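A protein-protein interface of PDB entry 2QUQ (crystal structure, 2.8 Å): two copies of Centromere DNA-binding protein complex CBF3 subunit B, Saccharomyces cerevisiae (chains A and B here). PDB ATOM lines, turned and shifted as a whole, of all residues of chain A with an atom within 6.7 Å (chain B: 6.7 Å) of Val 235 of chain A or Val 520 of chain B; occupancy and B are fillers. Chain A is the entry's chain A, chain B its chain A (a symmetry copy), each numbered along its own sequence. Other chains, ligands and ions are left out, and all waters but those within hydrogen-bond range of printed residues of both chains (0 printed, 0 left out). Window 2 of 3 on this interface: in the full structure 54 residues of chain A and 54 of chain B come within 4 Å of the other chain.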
ATOM      1  N   ASP A 232     -25.999   0.347 -26.411  1.00  0.00           N
ATOM      2  CA  ASP A 232     -26.131   1.759 -26.076  1.00  0.00           C
ATOM      3  C   ASP A 232     -27.421   2.209 -26.772  1.00  0.00           C
ATOM      4  O   ASP A 232     -27.732   1.697 -27.850  1.00  0.00           O
ATOM      5  CB  ASP A 232     -24.940   2.519 -26.668  1.00  0.00           C
ATOM      6  CG  ASP A 232     -24.328   3.506 -25.704  1.00  0.00           C
ATOM      7  OD1 ASP A 232     -25.074   4.094 -24.894  1.00  0.00           O
ATOM      8  OD2 ASP A 232     -23.094   3.700 -25.777  1.00  0.00           O
ATOM      9  N   ASP A 233     -28.178   3.139 -26.187  1.00  0.00           N
ATOM     10  CA  ASP A 233     -29.399   3.600 -26.859  1.00  0.00           C
ATOM     11  C   ASP A 233     -28.975   4.322 -28.139  1.00  0.00           C
ATOM     12  O   ASP A 233     -28.190   5.270 -28.083  1.00  0.00           O
ATOM     13  CB  ASP A 233     -30.202   4.557 -25.969  1.00  0.00           C
ATOM     14  CG  ASP A 233     -31.446   5.102 -26.669  1.00  0.00           C
ATOM     15  OD1 ASP A 233     -32.262   4.297 -27.167  1.00  0.00           O
ATOM     16  OD2 ASP A 233     -31.615   6.340 -26.722  1.00  0.00           O
ATOM     17  N   PRO A 234     -29.490   3.892 -29.310  1.00  0.00           N
ATOM     18  CA  PRO A 234     -29.121   4.531 -30.577  1.00  0.00           C
ATOM     19  C   PRO A 234     -29.055   6.061 -30.557  1.00  0.00           C
ATOM     20  O   PRO A 234     -28.257   6.648 -31.277  1.00  0.00           O
ATOM     21  CB  PRO A 234     -30.156   3.982 -31.559  1.00  0.00           C
ATOM     22  CG  PRO A 234     -31.319   3.653 -30.687  1.00  0.00           C
ATOM     23  CD  PRO A 234     -30.657   3.016 -29.505  1.00  0.00           C
ATOM     24  N   VAL A 235     -29.877   6.708 -29.737  1.00  0.00           N
ATOM     25  CA  VAL A 235     -29.840   8.166 -29.642  1.00  0.00           C
ATOM     26  C   VAL A 235     -28.476   8.605 -29.111  1.00  0.00           C
ATOM     27  O   VAL A 235     -27.846   9.540 -29.625  1.00  0.00           O
ATOM     28  CB  VAL A 235     -30.899   8.701 -28.666  1.00  0.00           C
ATOM     29  CG1 VAL A 235     -30.745  10.209 -28.512  1.00  0.00           C
ATOM     30  CG2 VAL A 235     -32.284   8.355 -29.164  1.00  0.00           C
ATOM     31  N   GLU A 236     -28.040   7.922 -28.058  1.00  0.00           N
ATOM     32  CA  GLU A 236     -26.769   8.196 -27.420  1.00  0.00           C
ATOM     33  C   GLU A 236     -25.615   7.715 -28.304  1.00  0.00           C
ATOM     34  O   GLU A 236     -24.589   8.375 -28.392  1.00  0.00           O
ATOM     35  CB  GLU A 236     -26.728   7.493 -26.077  1.00  0.00           C
ATOM     36  CG  GLU A 236     -25.740   8.077 -25.119  1.00  0.00           C
ATOM     37  CD  GLU A 236     -25.598   7.227 -23.886  1.00  0.00           C
ATOM     38  OE1 GLU A 236     -26.645   6.857 -23.306  1.00  0.00           O
ATOM     39  OE2 GLU A 236     -24.444   6.932 -23.501  1.00  0.00           O
ATOM     40  N   SER A 237     -25.773   6.567 -28.957  1.00  0.00           N
ATOM     41  CA  SER A 237     -24.723   6.053 -29.841  1.00  0.00           C
ATOM     42  C   SER A 237     -24.445   7.091 -30.920  1.00  0.00           C
ATOM     43  O   SER A 237     -23.322   7.236 -31.398  1.00  0.00           O
ATOM     44  CB  SER A 237     -25.174   4.769 -30.528  1.00  0.00           C
ATOM     45  OG  SER A 237     -25.605   3.809 -29.595  1.00  0.00           O
ATOM     46  N   ILE A 238     -25.489   7.805 -31.306  1.00  0.00           N
ATOM     47  CA  ILE A 238     -25.366   8.818 -32.332  1.00  0.00           C
ATOM     48  C   ILE A 238     -24.666  10.048 -31.787  1.00  0.00           C
ATOM     49  O   ILE A 238     -23.750  10.566 -32.430  1.00  0.00           O
ATOM     50  CB  ILE A 238     -26.752   9.195 -32.903  1.00  0.00           C
ATOM     51  CG1 ILE A 238     -27.288   8.029 -33.739  1.00  0.00           C
ATOM     52  CG2 ILE A 238     -26.657  10.438 -33.756  1.00  0.00           C
ATOM     53  CD1 ILE A 238     -28.741   8.175 -34.145  1.00  0.00           C
ATOM     54  N   ALA A 239     -25.081  10.509 -30.607  1.00  0.00           N
ATOM     55  CA  ALA A 239     -24.469  11.692 -29.983  1.00  0.00           C
ATOM     56  C   ALA A 239     -22.959  11.509 -29.760  1.00  0.00           C
ATOM     57  O   ALA A 239     -22.180  12.445 -29.925  1.00  0.00           O
ATOM     58  CB  ALA A 239     -25.166  12.022 -28.651  1.00  0.00           C
ATOM     59  N   LYS A 240     -22.552  10.305 -29.375  1.00  0.00           N
ATOM     60  CA  LYS A 240     -21.147  10.017 -29.167  1.00  0.00           C
ATOM     61  C   LYS A 240     -20.444  10.151 -30.513  1.00  0.00           C
ATOM     62  O   LYS A 240     -19.471  10.877 -30.623  1.00  0.00           O
ATOM     63  CB  LYS A 240     -20.972   8.601 -28.602  1.00  0.00           C
ATOM     64  CG  LYS A 240     -21.393   8.464 -27.145  1.00  0.00           C
ATOM     65  CD  LYS A 240     -21.404   7.015 -26.688  1.00  0.00           C
ATOM     66  CE  LYS A 240     -20.037   6.363 -26.838  1.00  0.00           C
ATOM     67  NZ  LYS A 240     -20.043   4.924 -26.413  1.00  0.00           N
ATOM     68  N   MET B 509     -24.421  13.834 -20.422  1.00  0.00           N
ATOM     69  CA  MET B 509     -24.828  13.167 -21.645  1.00  0.00           C
ATOM     70  C   MET B 509     -26.227  13.532 -22.111  1.00  0.00           C
ATOM     71  O   MET B 509     -26.499  13.496 -23.314  1.00  0.00           O
ATOM     72  CB  MET B 509     -24.712  11.654 -21.499  1.00  0.00           C
ATOM     73  CG  MET B 509     -25.145  10.901 -22.746  1.00  0.00           C
ATOM     74  SD  MET B 509     -24.385  11.505 -24.293  1.00  0.00           S
ATOM     75  CE  MET B 509     -23.132  10.211 -24.629  1.00  0.00           C
ATOM     76  N   PHE B 510     -27.135  13.873 -21.199  1.00  0.00           N
ATOM     77  CA  PHE B 510     -28.453  14.249 -21.687  1.00  0.00           C
ATOM     78  C   PHE B 510     -28.345  15.668 -22.221  1.00  0.00           C
ATOM     79  O   PHE B 510     -28.940  15.998 -23.240  1.00  0.00           O
ATOM     80  CB  PHE B 510     -29.543  14.155 -20.610  1.00  0.00           C
ATOM     81  CG  PHE B 510     -30.889  13.713 -21.160  1.00  0.00           C
ATOM     82  CD1 PHE B 510     -31.501  14.420 -22.196  1.00  0.00           C
ATOM     83  CD2 PHE B 510     -31.515  12.562 -20.679  1.00  0.00           C
ATOM     84  CE1 PHE B 510     -32.713  13.985 -22.750  1.00  0.00           C
ATOM     85  CE2 PHE B 510     -32.728  12.118 -21.227  1.00  0.00           C
ATOM     86  CZ  PHE B 510     -33.326  12.833 -22.265  1.00  0.00           C
ATOM     87  N   ILE B 513     -27.178  15.493 -25.600  1.00  0.00           N
ATOM     88  CA  ILE B 513     -28.249  15.043 -26.461  1.00  0.00           C
ATOM     89  C   ILE B 513     -29.254  16.153 -26.808  1.00  0.00           C
ATOM     90  O   ILE B 513     -29.837  16.129 -27.877  1.00  0.00           O
ATOM     91  CB  ILE B 513     -28.947  13.816 -25.821  1.00  0.00           C
ATOM     92  CG1 ILE B 513     -28.042  12.594 -25.979  1.00  0.00           C
ATOM     93  CG2 ILE B 513     -30.304  13.566 -26.452  1.00  0.00           C
ATOM     94  CD1 ILE B 513     -28.660  11.296 -25.513  1.00  0.00           C
ATOM     95  N   LYS B 514     -29.439  17.138 -25.934  1.00  0.00           N
ATOM     96  CA  LYS B 514     -30.383  18.228 -26.214  1.00  0.00           C
ATOM     97  C   LYS B 514     -29.773  19.337 -27.066  1.00  0.00           C
ATOM     98  O   LYS B 514     -30.474  19.944 -27.872  1.00  0.00           O
ATOM     99  CB  LYS B 514     -30.908  18.860 -24.922  1.00  0.00           C
ATOM    100  CG  LYS B 514     -31.713  17.926 -24.021  1.00  0.00           C
ATOM    101  CD  LYS B 514     -32.118  18.638 -22.728  1.00  0.00           C
ATOM    102  CE  LYS B 514     -32.556  17.660 -21.646  1.00  0.00           C
ATOM    103  NZ  LYS B 514     -32.767  18.357 -20.345  1.00  0.00           N
ATOM    104  N   GLY B 517     -28.566  17.150 -32.328  1.00  0.00           N
ATOM    105  CA  GLY B 517     -29.691  16.882 -33.222  1.00  0.00           C
ATOM    106  C   GLY B 517     -31.070  16.853 -32.587  1.00  0.00           C
ATOM    107  O   GLY B 517     -32.056  16.453 -33.217  1.00  0.00           O
ATOM    108  N   SER B 518     -31.113  17.263 -31.325  1.00  0.00           N
ATOM    109  CA  SER B 518     -32.327  17.357 -30.527  1.00  0.00           C
ATOM    110  C   SER B 518     -33.228  16.132 -30.413  1.00  0.00           C
ATOM    111  O   SER B 518     -34.322  16.229 -29.852  1.00  0.00           O
ATOM    112  CB  SER B 518     -33.152  18.555 -31.000  1.00  0.00           C
ATOM    113  OG  SER B 518     -33.351  18.489 -32.403  1.00  0.00           O
ATOM    114  N   LEU B 519     -32.794  14.985 -30.939  1.00  0.00           N
ATOM    115  CA  LEU B 519     -33.584  13.759 -30.807  1.00  0.00           C
ATOM    116  C   LEU B 519     -33.661  13.619 -29.276  1.00  0.00           C
ATOM    117  O   LEU B 519     -33.198  14.510 -28.561  1.00  0.00           O
ATOM    118  CB  LEU B 519     -32.834  12.557 -31.414  1.00  0.00           C
ATOM    119  CG  LEU B 519     -32.479  12.461 -32.910  1.00  0.00           C
ATOM    120  CD1 LEU B 519     -31.452  11.352 -33.107  1.00  0.00           C
ATOM    121  CD2 LEU B 519     -33.722  12.177 -33.748  1.00  0.00           C
ATOM    122  N   VAL B 520     -34.219  12.536 -28.747  1.00  0.00           N
ATOM    123  CA  VAL B 520     -34.283  12.421 -27.285  1.00  0.00           C
ATOM    124  C   VAL B 520     -33.994  11.007 -26.775  1.00  0.00           C
ATOM    125  O   VAL B 520     -33.490  10.824 -25.662  1.00  0.00           O
ATOM    126  CB  VAL B 520     -35.670  12.882 -26.739  1.00  0.00           C
ATOM    127  CG1 VAL B 520     -35.614  13.026 -25.214  1.00  0.00           C
ATOM    128  CG2 VAL B 520     -36.084  14.200 -27.384  1.00  0.00           C
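Among the printed residues, pairs that only touch across the chains: Val 235 of chain A with Ile 513 of chain B (3.8 Å), Val 235 of chain A with Val 520 of chain B (3.8 Å), Glu 236 of chain A with Met 509 of chain B (3.4 Å), Ala 239 of chain A with Ile 513 of chain B (3.97 Å) and Lys 240 of chain A with Met 509 of chain B (3.5 Å).
No position is printed for both chains.
OD2 of Asp 232 of chain A is in salt-bridge range of NZ of Lys 240 of chain A (3.3 Å).
The backbone NH (N) of Val 235 of chain A sits close to the side-chain carboxylate (OD2) of Asp 233 of chain A.
Of chain B, only Ile 513 (3.8 Å) and Val 520 (3.8 Å) come within 4 Å of Val 235 of chain A.
Of the printed residues of chain A, Val 520 of chain B touches Val 235.
Of the printed residues of chain A, Ile 513 of chain B touches Val 235 (3.8 Å) and Ala 239 (3.97 Å).
Printed residues of chain B within 4 Å of Lys 240 of chain A: Met 509 (3.5 Å).
Printed residues of chain A within 4 Å of Met 509 of chain B: Glu 236 and Lys 240.
Of the printed residues of chain B, Ala 239 of chain A touches Ile 513.
The nearest residue of chain A that does not touch Val 520 of chain B is Asp 233 of chain A (5.0 Å).
Of the 8 printed residues of chain B, 3 touch a printed residue of chain A.
Printed residues of chain B that touch a printed residue of chain A: Met 509, Ile 513 and Val 520.
Hydrophobic or aromatic side chains of chain B that line the printed part of chain A: Met 509 and Ile 513.
Hydrophobic or aromatic side chains of chain A within 4 Å of the printed part of chain B: Val 235 and Ala 239.
Among the printed residues, no Asp or Glu carboxylate lies within 4 Å of a Lys or Arg side-chain nitrogen of the other chain.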
